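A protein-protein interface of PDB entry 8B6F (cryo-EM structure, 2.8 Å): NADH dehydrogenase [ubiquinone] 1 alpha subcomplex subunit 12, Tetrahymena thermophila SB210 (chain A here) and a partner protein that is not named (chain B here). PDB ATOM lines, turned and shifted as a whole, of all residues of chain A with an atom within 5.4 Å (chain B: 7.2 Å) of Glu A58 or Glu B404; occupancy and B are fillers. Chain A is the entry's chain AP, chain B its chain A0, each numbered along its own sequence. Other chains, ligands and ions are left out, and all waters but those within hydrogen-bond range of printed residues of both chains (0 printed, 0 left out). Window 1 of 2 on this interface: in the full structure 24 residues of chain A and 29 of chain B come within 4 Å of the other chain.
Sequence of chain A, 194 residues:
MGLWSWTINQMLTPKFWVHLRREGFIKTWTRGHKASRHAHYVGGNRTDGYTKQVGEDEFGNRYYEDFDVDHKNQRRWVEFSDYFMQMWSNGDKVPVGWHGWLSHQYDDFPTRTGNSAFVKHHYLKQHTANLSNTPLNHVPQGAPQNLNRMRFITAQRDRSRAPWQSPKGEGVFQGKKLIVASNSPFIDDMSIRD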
ATOM      1  N   LYS A  27      13.816  17.302  -3.277  1.00  0.00           N
ATOM      2  CA  LYS A  27      14.222  17.600  -4.645  1.00  0.00           C
ATOM      3  C   LYS A  27      14.193  19.098  -4.915  1.00  0.00           C
ATOM      4  O   LYS A  27      15.145  19.658  -5.467  1.00  0.00           O
ATOM      5  CB  LYS A  27      13.317  16.859  -5.629  1.00  0.00           C
ATOM      6  CG  LYS A  27      13.475  15.349  -5.603  1.00  0.00           C
ATOM      7  CD  LYS A  27      14.827  14.927  -6.157  1.00  0.00           C
ATOM      8  CE  LYS A  27      14.926  13.415  -6.272  1.00  0.00           C
ATOM      9  NZ  LYS A  27      16.218  12.991  -6.881  1.00  0.00           N
ATOM     10  N   GLU A  56      17.199  13.474 -19.039  1.00  0.00           N
ATOM     11  CA  GLU A  56      18.154  13.024 -18.041  1.00  0.00           C
ATOM     12  C   GLU A  56      19.107  12.027 -18.678  1.00  0.00           C
ATOM     13  O   GLU A  56      18.728  11.268 -19.573  1.00  0.00           O
ATOM     14  CB  GLU A  56      17.441  12.397 -16.833  1.00  0.00           C
ATOM     15  CG  GLU A  56      16.537  11.219 -17.177  1.00  0.00           C
ATOM     16  CD  GLU A  56      17.288   9.907 -17.272  1.00  0.00           C
ATOM     17  OE1 GLU A  56      18.340   9.771 -16.616  1.00  0.00           O
ATOM     18  OE2 GLU A  56      16.824   9.008 -18.003  1.00  0.00           O
ATOM     19  N   ASP A  57      20.352  12.039 -18.213  1.00  0.00           N
ATOM     20  CA  ASP A  57      21.398  11.206 -18.779  1.00  0.00           C
ATOM     21  C   ASP A  57      21.601   9.955 -17.927  1.00  0.00           C
ATOM     22  O   ASP A  57      20.900   9.711 -16.944  1.00  0.00           O
ATOM     23  CB  ASP A  57      22.698  11.999 -18.911  1.00  0.00           C
ATOM     24  CG  ASP A  57      23.283  12.385 -17.575  1.00  0.00           C
ATOM     25  OD1 ASP A  57      22.525  12.424 -16.584  1.00  0.00           O
ATOM     26  OD2 ASP A  57      24.500  12.653 -17.512  1.00  0.00           O
ATOM     27  N   GLU A  58      22.588   9.148 -18.322  1.00  0.00           N
ATOM     28  CA  GLU A  58      22.826   7.871 -17.662  1.00  0.00           C
ATOM     29  C   GLU A  58      23.344   8.028 -16.240  1.00  0.00           C
ATOM     30  O   GLU A  58      23.254   7.078 -15.456  1.00  0.00           O
ATOM     31  CB  GLU A  58      23.816   7.044 -18.482  1.00  0.00           C
ATOM     32  CG  GLU A  58      23.268   6.603 -19.828  1.00  0.00           C
ATOM     33  CD  GLU A  58      24.239   5.728 -20.591  1.00  0.00           C
ATOM     34  OE1 GLU A  58      25.366   5.519 -20.095  1.00  0.00           O
ATOM     35  OE2 GLU A  58      23.877   5.247 -21.685  1.00  0.00           O
ATOM     36  N   PHE A  59      23.883   9.192 -15.889  1.00  0.00           N
ATOM     37  CA  PHE A  59      24.456   9.422 -14.571  1.00  0.00           C
ATOM     38  C   PHE A  59      23.521  10.195 -13.652  1.00  0.00           C
ATOM     39  O   PHE A  59      23.955  10.663 -12.596  1.00  0.00           O
ATOM     40  CB  PHE A  59      25.789  10.158 -14.701  1.00  0.00           C
ATOM     41  CG  PHE A  59      26.791   9.440 -15.558  1.00  0.00           C
ATOM     42  CD1 PHE A  59      27.598   8.451 -15.022  1.00  0.00           C
ATOM     43  CD2 PHE A  59      26.919   9.750 -16.900  1.00  0.00           C
ATOM     44  CE1 PHE A  59      28.518   7.787 -15.808  1.00  0.00           C
ATOM     45  CE2 PHE A  59      27.836   9.089 -17.693  1.00  0.00           C
ATOM     46  CZ  PHE A  59      28.637   8.107 -17.147  1.00  0.00           C
ATOM     47  N   GLY A  60      22.253  10.342 -14.027  1.00  0.00           N
ATOM     48  CA  GLY A  60      21.282  11.014 -13.193  1.00  0.00           C
ATOM     49  C   GLY A  60      21.249  12.520 -13.320  1.00  0.00           C
ATOM     50  O   GLY A  60      20.457  13.162 -12.621  1.00  0.00           O
ATOM     51  N   ARG A  62      20.244  16.117 -14.738  1.00  0.00           N
ATOM     52  CA  ARG A  62      19.027  16.643 -15.342  1.00  0.00           C
ATOM     53  C   ARG A  62      19.353  17.910 -16.116  1.00  0.00           C
ATOM     54  O   ARG A  62      19.964  18.834 -15.569  1.00  0.00           O
ATOM     55  CB  ARG A  62      17.971  16.936 -14.274  1.00  0.00           C
ATOM     56  CG  ARG A  62      17.686  15.770 -13.340  1.00  0.00           C
ATOM     57  CD  ARG A  62      17.145  14.574 -14.097  1.00  0.00           C
ATOM     58  NE  ARG A  62      16.934  13.424 -13.228  1.00  0.00           N
ATOM     59  CZ  ARG A  62      15.851  13.223 -12.492  1.00  0.00           C
ATOM     60  NH1 ARG A  62      14.855  14.094 -12.475  1.00  0.00           N
ATOM     61  NH2 ARG A  62      15.762  12.121 -11.754  1.00  0.00           N
ATOM     62  N   PRO A  95      27.955  13.577 -20.253  1.00  0.00           N
ATOM     63  CA  PRO A  95      28.191  12.493 -21.213  1.00  0.00           C
ATOM     64  C   PRO A  95      28.382  13.023 -22.626  1.00  0.00           C
ATOM     65  O   PRO A  95      28.230  14.211 -22.914  1.00  0.00           O
ATOM     66  CB  PRO A  95      26.929  11.633 -21.101  1.00  0.00           C
ATOM     67  CG  PRO A  95      26.385  11.938 -19.765  1.00  0.00           C
ATOM     68  CD  PRO A  95      26.694  13.379 -19.519  1.00  0.00           C
ATOM     69  N   ARG A 112      16.305   8.451 -24.450  1.00  0.00           N
ATOM     70  CA  ARG A 112      16.298   7.041 -24.097  1.00  0.00           C
ATOM     71  C   ARG A 112      14.997   6.406 -24.565  1.00  0.00           C
ATOM     72  O   ARG A 112      13.915   6.964 -24.356  1.00  0.00           O
ATOM     73  CB  ARG A 112      16.468   6.872 -22.585  1.00  0.00           C
ATOM     74  CG  ARG A 112      15.272   7.338 -21.757  1.00  0.00           C
ATOM     75  CD  ARG A 112      15.465   7.030 -20.283  1.00  0.00           C
ATOM     76  NE  ARG A 112      14.215   7.120 -19.539  1.00  0.00           N
ATOM     77  CZ  ARG A 112      14.079   6.805 -18.258  1.00  0.00           C
ATOM     78  NH1 ARG A 112      15.105   6.379 -17.538  1.00  0.00           N
ATOM     79  NH2 ARG A 112      12.887   6.923 -17.683  1.00  0.00           N
ATOM     80  N   GLN A 126      30.622   3.203 -22.233  1.00  0.00           N
ATOM     81  CA  GLN A 126      30.005   4.244 -21.425  1.00  0.00           C
ATOM     82  C   GLN A 126      30.985   5.384 -21.174  1.00  0.00           C
ATOM     83  O   GLN A 126      32.191   5.177 -21.024  1.00  0.00           O
ATOM     84  CB  GLN A 126      29.515   3.674 -20.094  1.00  0.00           C
ATOM     85  CG  GLN A 126      28.728   4.673 -19.257  1.00  0.00           C
ATOM     86  CD  GLN A 126      28.155   4.058 -17.996  1.00  0.00           C
ATOM     87  OE1 GLN A 126      28.488   2.932 -17.632  1.00  0.00           O
ATOM     88  NE2 GLN A 126      27.282   4.799 -17.323  1.00  0.00           N
ATOM     89  N   HIS A 127      30.449   6.599 -21.124  1.00  0.00           N
ATOM     90  CA  HIS A 127      31.279   7.773 -20.901  1.00  0.00           C
ATOM     91  C   HIS A 127      31.912   7.722 -19.518  1.00  0.00           C
ATOM     92  O   HIS A 127      31.311   7.233 -18.557  1.00  0.00           O
ATOM     93  CB  HIS A 127      30.437   9.040 -21.054  1.00  0.00           C
ATOM     94  CG  HIS A 127      31.182  10.303 -20.752  1.00  0.00           C
ATOM     95  ND1 HIS A 127      31.164  10.896 -19.508  1.00  0.00           N
ATOM     96  CD2 HIS A 127      31.958  11.090 -21.533  1.00  0.00           C
ATOM     97  CE1 HIS A 127      31.899  11.992 -19.535  1.00  0.00           C
ATOM     98  NE2 HIS A 127      32.392  12.134 -20.751  1.00  0.00           N
ATOM     99  N   ASN B 392      24.065   9.736  -3.364  1.00  0.00           N
ATOM    100  CA  ASN B 392      23.429  10.212  -4.588  1.00  0.00           C
ATOM    101  C   ASN B 392      22.469   9.180  -5.160  1.00  0.00           C
ATOM    102  O   ASN B 392      21.789   9.469  -6.150  1.00  0.00           O
ATOM    103  CB  ASN B 392      24.449  10.596  -5.668  1.00  0.00           C
ATOM    104  CG  ASN B 392      25.557  11.478  -5.133  1.00  0.00           C
ATOM    105  OD1 ASN B 392      26.737  11.158  -5.261  1.00  0.00           O
ATOM    106  ND2 ASN B 392      25.181  12.593  -4.517  1.00  0.00           N
ATOM    107  N   PHE B 393      22.386   7.991  -4.567  1.00  0.00           N
ATOM    108  CA  PHE B 393      21.506   6.932  -5.037  1.00  0.00           C
ATOM    109  C   PHE B 393      21.069   6.108  -3.835  1.00  0.00           C
ATOM    110  O   PHE B 393      21.722   6.107  -2.790  1.00  0.00           O
ATOM    111  CB  PHE B 393      22.198   6.043  -6.075  1.00  0.00           C
ATOM    112  CG  PHE B 393      22.733   6.798  -7.255  1.00  0.00           C
ATOM    113  CD1 PHE B 393      21.879   7.286  -8.229  1.00  0.00           C
ATOM    114  CD2 PHE B 393      24.094   7.019  -7.392  1.00  0.00           C
ATOM    115  CE1 PHE B 393      22.371   7.983  -9.317  1.00  0.00           C
ATOM    116  CE2 PHE B 393      24.593   7.715  -8.475  1.00  0.00           C
ATOM    117  CZ  PHE B 393      23.730   8.197  -9.440  1.00  0.00           C
ATOM    118  N   ASN B 398      21.341   0.825  -8.690  1.00  0.00           N
ATOM    119  CA  ASN B 398      21.589   2.195  -9.124  1.00  0.00           C
ATOM    120  C   ASN B 398      22.958   2.681  -8.665  1.00  0.00           C
ATOM    121  O   ASN B 398      23.684   3.327  -9.428  1.00  0.00           O
ATOM    122  CB  ASN B 398      20.493   3.123  -8.600  1.00  0.00           C
ATOM    123  CG  ASN B 398      19.203   3.000  -9.384  1.00  0.00           C
ATOM    124  OD1 ASN B 398      19.216   2.743 -10.585  1.00  0.00           O
ATOM    125  ND2 ASN B 398      18.080   3.186  -8.705  1.00  0.00           N
ATOM    126  N   PHE B 399      23.329   2.381  -7.420  1.00  0.00           N
ATOM    127  CA  PHE B 399      24.648   2.771  -6.932  1.00  0.00           C
ATOM    128  C   PHE B 399      25.748   2.020  -7.671  1.00  0.00           C
ATOM    129  O   PHE B 399      26.807   2.589  -7.960  1.00  0.00           O
ATOM    130  CB  PHE B 399      24.751   2.525  -5.428  1.00  0.00           C
ATOM    131  CG  PHE B 399      25.999   3.090  -4.810  1.00  0.00           C
ATOM    132  CD1 PHE B 399      26.026   4.395  -4.345  1.00  0.00           C
ATOM    133  CD2 PHE B 399      27.146   2.321  -4.695  1.00  0.00           C
ATOM    134  CE1 PHE B 399      27.170   4.921  -3.778  1.00  0.00           C
ATOM    135  CE2 PHE B 399      28.293   2.844  -4.129  1.00  0.00           C
ATOM    136  CZ  PHE B 399      28.304   4.145  -3.670  1.00  0.00           C
ATOM    137  N   ILE B 401      25.747   0.971 -10.789  1.00  0.00           N
ATOM    138  CA  ILE B 401      25.930   1.581 -12.107  1.00  0.00           C
ATOM    139  C   ILE B 401      26.227   3.067 -12.023  1.00  0.00           C
ATOM    140  O   ILE B 401      26.491   3.691 -13.058  1.00  0.00           O
ATOM    141  CB  ILE B 401      24.700   1.374 -13.015  1.00  0.00           C
ATOM    142  CG1 ILE B 401      23.473   2.098 -12.448  1.00  0.00           C
ATOM    143  CG2 ILE B 401      24.417  -0.106 -13.172  1.00  0.00           C
ATOM    144  CD1 ILE B 401      22.242   2.024 -13.332  1.00  0.00           C
ATOM    145  N   GLN B 402      26.191   3.657 -10.827  1.00  0.00           N
ATOM    146  CA  GLN B 402      26.411   5.092 -10.660  1.00  0.00           C
ATOM    147  C   GLN B 402      25.447   5.894 -11.530  1.00  0.00           C
ATOM    148  O   GLN B 402      25.817   6.902 -12.134  1.00  0.00           O
ATOM    149  CB  GLN B 402      27.862   5.466 -10.970  1.00  0.00           C
ATOM    150  CG  GLN B 402      28.882   4.887 -10.000  1.00  0.00           C
ATOM    151  CD  GLN B 402      28.844   5.550  -8.635  1.00  0.00           C
ATOM    152  OE1 GLN B 402      27.786   5.690  -8.025  1.00  0.00           O
ATOM    153  NE2 GLN B 402      30.009   5.966  -8.150  1.00  0.00           N
ATOM    154  N   GLY B 403      24.197   5.447 -11.586  1.00  0.00           N
ATOM    155  CA  GLY B 403      23.193   6.107 -12.397  1.00  0.00           C
ATOM    156  C   GLY B 403      21.805   5.725 -11.940  1.00  0.00           C
ATOM    157  O   GLY B 403      21.615   4.746 -11.214  1.00  0.00           O
ATOM    158  N   GLU B 404      20.830   6.516 -12.380  1.00  0.00           N
ATOM    159  CA  GLU B 404      19.433   6.360 -11.982  1.00  0.00           C
ATOM    160  C   GLU B 404      18.628   5.898 -13.194  1.00  0.00           C
ATOM    161  O   GLU B 404      18.066   6.710 -13.930  1.00  0.00           O
ATOM    162  CB  GLU B 404      18.886   7.671 -11.419  1.00  0.00           C
ATOM    163  CG  GLU B 404      17.443   7.590 -10.943  1.00  0.00           C
ATOM    164  CD  GLU B 404      16.896   8.938 -10.513  1.00  0.00           C
ATOM    165  OE1 GLU B 404      17.640   9.936 -10.604  1.00  0.00           O
ATOM    166  OE2 GLU B 404      15.724   9.001 -10.087  1.00  0.00           O
ATOM    167  N   ALA B 405      18.574   4.580 -13.398  1.00  0.00           N
ATOM    168  CA  ALA B 405      17.714   4.017 -14.433  1.00  0.00           C
ATOM    169  C   ALA B 405      16.281   3.878 -13.929  1.00  0.00           C
ATOM    170  O   ALA B 405      15.353   4.475 -14.484  1.00  0.00           O
ATOM    171  CB  ALA B 405      18.261   2.666 -14.894  1.00  0.00           C
ATOM    172  N   TYR B 406      16.085   3.091 -12.873  1.00  0.00           N
ATOM    173  CA  TYR B 406      14.808   3.050 -12.173  1.00  0.00           C
ATOM    174  C   TYR B 406      14.702   4.286 -11.291  1.00  0.00           C
ATOM    175  O   TYR B 406      15.489   4.452 -10.353  1.00  0.00           O
ATOM    176  CB  TYR B 406      14.689   1.785 -11.324  1.00  0.00           C
ATOM    177  CG  TYR B 406      14.569   0.486 -12.093  1.00  0.00           C
ATOM    178  CD1 TYR B 406      14.267   0.473 -13.449  1.00  0.00           C
ATOM    179  CD2 TYR B 406      14.742  -0.733 -11.450  1.00  0.00           C
ATOM    180  CE1 TYR B 406      14.152  -0.718 -14.142  1.00  0.00           C
ATOM    181  CE2 TYR B 406      14.628  -1.926 -12.134  1.00  0.00           C
ATOM    182  CZ  TYR B 406      14.333  -1.912 -13.480  1.00  0.00           C
ATOM    183  OH  TYR B 406      14.220  -3.097 -14.168  1.00  0.00           O
ATOM    184  N   HIS B 407      13.739   5.153 -11.586  1.00  0.00           N
ATOM    185  CA  HIS B 407      13.586   6.374 -10.808  1.00  0.00           C
ATOM    186  C   HIS B 407      13.240   6.053  -9.361  1.00  0.00           C
ATOM    187  O   HIS B 407      12.408   5.187  -9.076  1.00  0.00           O
ATOM    188  CB  HIS B 407      12.515   7.266 -11.430  1.00  0.00           C
ATOM    189  CG  HIS B 407      12.955   7.934 -12.696  1.00  0.00           C
ATOM    190  ND1 HIS B 407      14.173   7.675 -13.288  1.00  0.00           N
ATOM    191  CD2 HIS B 407      12.345   8.854 -13.479  1.00  0.00           C
ATOM    192  CE1 HIS B 407      14.293   8.405 -14.381  1.00  0.00           C
ATOM    193  NE2 HIS B 407      13.197   9.129 -14.521  1.00  0.00           N
ATOM    194  N   GLU B 408      13.898   6.757  -8.445  1.00  0.00           N
ATOM    195  CA  GLU B 408      13.792   6.514  -7.014  1.00  0.00           C
ATOM    196  C   GLU B 408      12.988   7.633  -6.365  1.00  0.00           C
ATOM    197  O   GLU B 408      13.233   8.814  -6.632  1.00  0.00           O
ATOM    198  CB  GLU B 408      15.182   6.427  -6.381  1.00  0.00           C
ATOM    199  CG  GLU B 408      16.089   5.387  -7.032  1.00  0.00           C
ATOM    200  CD  GLU B 408      17.557   5.609  -6.721  1.00  0.00           C
ATOM    201  OE1 GLU B 408      17.939   6.763  -6.432  1.00  0.00           O
ATOM    202  OE2 GLU B 408      18.332   4.631  -6.767  1.00  0.00           O
ATOM    203  N   LEU B 409      12.038   7.259  -5.512  1.00  0.00           N
ATOM    204  CA  LEU B 409      11.164   8.198  -4.821  1.00  0.00           C
ATOM    205  C   LEU B 409      11.286   7.925  -3.329  1.00  0.00           C
ATOM    206  O   LEU B 409      10.904   6.845  -2.868  1.00  0.00           O
ATOM    207  CB  LEU B 409       9.717   8.037  -5.290  1.00  0.00           C
ATOM    208  CG  LEU B 409       9.516   8.024  -6.809  1.00  0.00           C
ATOM    209  CD1 LEU B 409       8.051   7.802  -7.148  1.00  0.00           C
ATOM    210  CD2 LEU B 409      10.026   9.298  -7.459  1.00  0.00           C
ATOM    211  N   LYS B 418       4.024  12.668  -8.129  1.00  0.00           N
ATOM    212  CA  LYS B 418       5.251  12.193  -8.756  1.00  0.00           C
ATOM    213  C   LYS B 418       5.150  10.720  -9.137  1.00  0.00           C
ATOM    214  O   LYS B 418       5.555  10.328 -10.236  1.00  0.00           O
ATOM    215  CB  LYS B 418       6.434  12.422  -7.817  1.00  0.00           C
ATOM    216  CG  LYS B 418       7.799  12.210  -8.456  1.00  0.00           C
ATOM    217  CD  LYS B 418       8.093  13.266  -9.512  1.00  0.00           C
ATOM    218  CE  LYS B 418       9.512  13.147 -10.040  1.00  0.00           C
ATOM    219  NZ  LYS B 418      10.528  13.390  -8.979  1.00  0.00           N
ATOM    220  N   GLU B 422       5.494   9.062 -12.884  1.00  0.00           N
ATOM    221  CA  GLU B 422       6.457   8.029 -13.251  1.00  0.00           C
ATOM    222  C   GLU B 422       5.755   6.786 -13.783  1.00  0.00           C
ATOM    223  O   GLU B 422       6.211   6.179 -14.758  1.00  0.00           O
ATOM    224  CB  GLU B 422       7.337   7.680 -12.052  1.00  0.00           C
ATOM    225  CG  GLU B 422       8.125   8.858 -11.495  1.00  0.00           C
ATOM    226  CD  GLU B 422       9.088   9.453 -12.502  1.00  0.00           C
ATOM    227  OE1 GLU B 422       9.308   8.830 -13.561  1.00  0.00           O
ATOM    228  OE2 GLU B 422       9.628  10.546 -12.234  1.00  0.00           O
ATOM    229  N   HIS B 435      15.576  -1.007 -22.655  1.00  0.00           N
ATOM    230  CA  HIS B 435      16.549  -0.024 -22.191  1.00  0.00           C
ATOM    231  C   HIS B 435      17.037  -0.359 -20.788  1.00  0.00           C
ATOM    232  O   HIS B 435      18.244  -0.352 -20.519  1.00  0.00           O
ATOM    233  CB  HIS B 435      15.925   1.371 -22.226  1.00  0.00           C
ATOM    234  CG  HIS B 435      16.820   2.448 -21.701  1.00  0.00           C
ATOM    235  ND1 HIS B 435      17.997   2.809 -22.321  1.00  0.00           N
ATOM    236  CD2 HIS B 435      16.708   3.250 -20.616  1.00  0.00           C
ATOM    237  CE1 HIS B 435      18.572   3.783 -21.641  1.00  0.00           C
ATOM    238  NE2 HIS B 435      17.810   4.070 -20.600  1.00  0.00           N
ATOM    239  N   PHE B 436      16.112  -0.663 -19.879  1.00  0.00           N
ATOM    240  CA  PHE B 436      16.502  -0.995 -18.512  1.00  0.00           C
ATOM    241  C   PHE B 436      17.263  -2.314 -18.457  1.00  0.00           C
ATOM    242  O   PHE B 436      18.214  -2.454 -17.682  1.00  0.00           O
ATOM    243  CB  PHE B 436      15.270  -1.046 -17.611  1.00  0.00           C
ATOM    244  CG  PHE B 436      14.594   0.285 -17.428  1.00  0.00           C
ATOM    245  CD1 PHE B 436      15.329   1.458 -17.383  1.00  0.00           C
ATOM    246  CD2 PHE B 436      13.218   0.359 -17.303  1.00  0.00           C
ATOM    247  CE1 PHE B 436      14.706   2.677 -17.214  1.00  0.00           C
ATOM    248  CE2 PHE B 436      12.589   1.577 -17.134  1.00  0.00           C
ATOM    249  CZ  PHE B 436      13.334   2.737 -17.089  1.00  0.00           C
ATOM    250  N   GLU B 438      19.250  -3.501 -20.786  1.00  0.00           N
ATOM    251  CA  GLU B 438      20.605  -3.182 -21.219  1.00  0.00           C
ATOM    252  C   GLU B 438      21.370  -2.444 -20.127  1.00  0.00           C
ATOM    253  O   GLU B 438      22.567  -2.679 -19.929  1.00  0.00           O
ATOM    254  CB  GLU B 438      20.560  -2.353 -22.502  1.00  0.00           C
ATOM    255  CG  GLU B 438      21.930  -2.065 -23.094  1.00  0.00           C
ATOM    256  CD  GLU B 438      21.848  -1.406 -24.457  1.00  0.00           C
ATOM    257  OE1 GLU B 438      20.727  -1.276 -24.990  1.00  0.00           O
ATOM    258  OE2 GLU B 438      22.906  -1.018 -24.995  1.00  0.00           O
ATOM    259  N   ARG B 439      20.694  -1.545 -19.410  1.00  0.00           N
ATOM    260  CA  ARG B 439      21.350  -0.796 -18.343  1.00  0.00           C
ATOM    261  C   ARG B 439      21.830  -1.713 -17.224  1.00  0.00           C
ATOM    262  O   ARG B 439      22.943  -1.548 -16.713  1.00  0.00           O
ATOM    263  CB  ARG B 439      20.392   0.262 -17.792  1.00  0.00           C
ATOM    264  CG  ARG B 439      20.144   1.414 -18.749  1.00  0.00           C
ATOM    265  CD  ARG B 439      21.290   2.406 -18.712  1.00  0.00           C
ATOM    266  NE  ARG B 439      21.203   3.286 -17.553  1.00  0.00           N
ATOM    267  CZ  ARG B 439      22.225   3.956 -17.040  1.00  0.00           C
ATOM    268  NH1 ARG B 439      23.447   3.838 -17.534  1.00  0.00           N
ATOM    269  NH2 ARG B 439      22.019   4.757 -16.000  1.00  0.00           N
ATOM    270  N   TYR B 440      21.008  -2.682 -16.829  1.00  0.00           N
ATOM    271  CA  TYR B 440      21.272  -3.513 -15.663  1.00  0.00           C
ATOM    272  C   TYR B 440      21.849  -4.879 -16.016  1.00  0.00           C
ATOM    273  O   TYR B 440      21.991  -5.722 -15.126  1.00  0.00           O
ATOM    274  CB  TYR B 440      19.986  -3.702 -14.855  1.00  0.00           C
ATOM    275  CG  TYR B 440      19.536  -2.474 -14.097  1.00  0.00           C
ATOM    276  CD1 TYR B 440      20.432  -1.729 -13.344  1.00  0.00           C
ATOM    277  CD2 TYR B 440      18.210  -2.065 -14.133  1.00  0.00           C
ATOM    278  CE1 TYR B 440      20.021  -0.612 -12.651  1.00  0.00           C
ATOM    279  CE2 TYR B 440      17.790  -0.949 -13.441  1.00  0.00           C
ATOM    280  CZ  TYR B 440      18.700  -0.228 -12.702  1.00  0.00           C
ATOM    281  OH  TYR B 440      18.287   0.886 -12.014  1.00  0.00           O
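Of chain B, only Gly B403, Glu B404 and Arg B439 come within 4 Å of Glu A58.
Of chain A, only Glu A58 (3.96 Å) and Arg A62 (3.1 Å) come within 4 Å of Glu B404.
Of the printed residues of chain B, Arg A112 touches Ala B405, His B407, His B435 and Phe B436.
Of the printed residues of chain A, Gln B402 touches Phe A59.
Ile B401 touches none of the printed residues of chain A.
The nearest residue of chain B that does not touch Glu A58 is Gln B402 (4.2 Å).
The nearest printed residue of chain B that does not touch Arg A62 is His B407 (4.8 Å).
The guanidinium group (NH2) of Arg A62 is in salt-bridge range of the side-chain carboxylate (OE1) of Glu B404 (3.1 Å).
The guanidinium group (NH1) of Arg B439 is in salt-bridge range of the side-chain carboxylate (OE1) of Glu A58, at 3.6 Å.
The side-chain amide nitrogen of Gln A126 lies within hydrogen-bond range of the side-chain carboxylate of Glu A58, 3.4 Å away.
The guanidinium group (NH1) of Arg A112 lies within salt-bridge range of the side-chain carboxylate (OE2) of Glu A56, at 3.2 Å.
The side-chain carboxylate (OE2) of Glu B404 is in hydrogen-bond range of the backbone NH (N) of Glu B408 (3.3 Å).
O of Phe B399 lies close to OE1 of Gln B402, 3.3 Å away.
OD1 of Asn B398 is in hydrogen-bond range of N of Ala B405.
O of Asn B398 is in hydrogen-bond range of N of Gly B403 (3.1 Å).
Hydrophobic or aromatic side chains of chain A that line the printed part of chain B: Phe A59.
Among the printed residues, 10 pairs touch across the chains.
Among the printed residues, pairs that only touch across the chains: Glu A58 with Gly B403, Glu A58 with Glu B404, Phe A59 with Gln B402, Arg A112 with Ala B405, Arg A112 with His B407, Arg A112 with His B435, Arg A112 with Phe B436 and Gln A126 with Arg B439.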
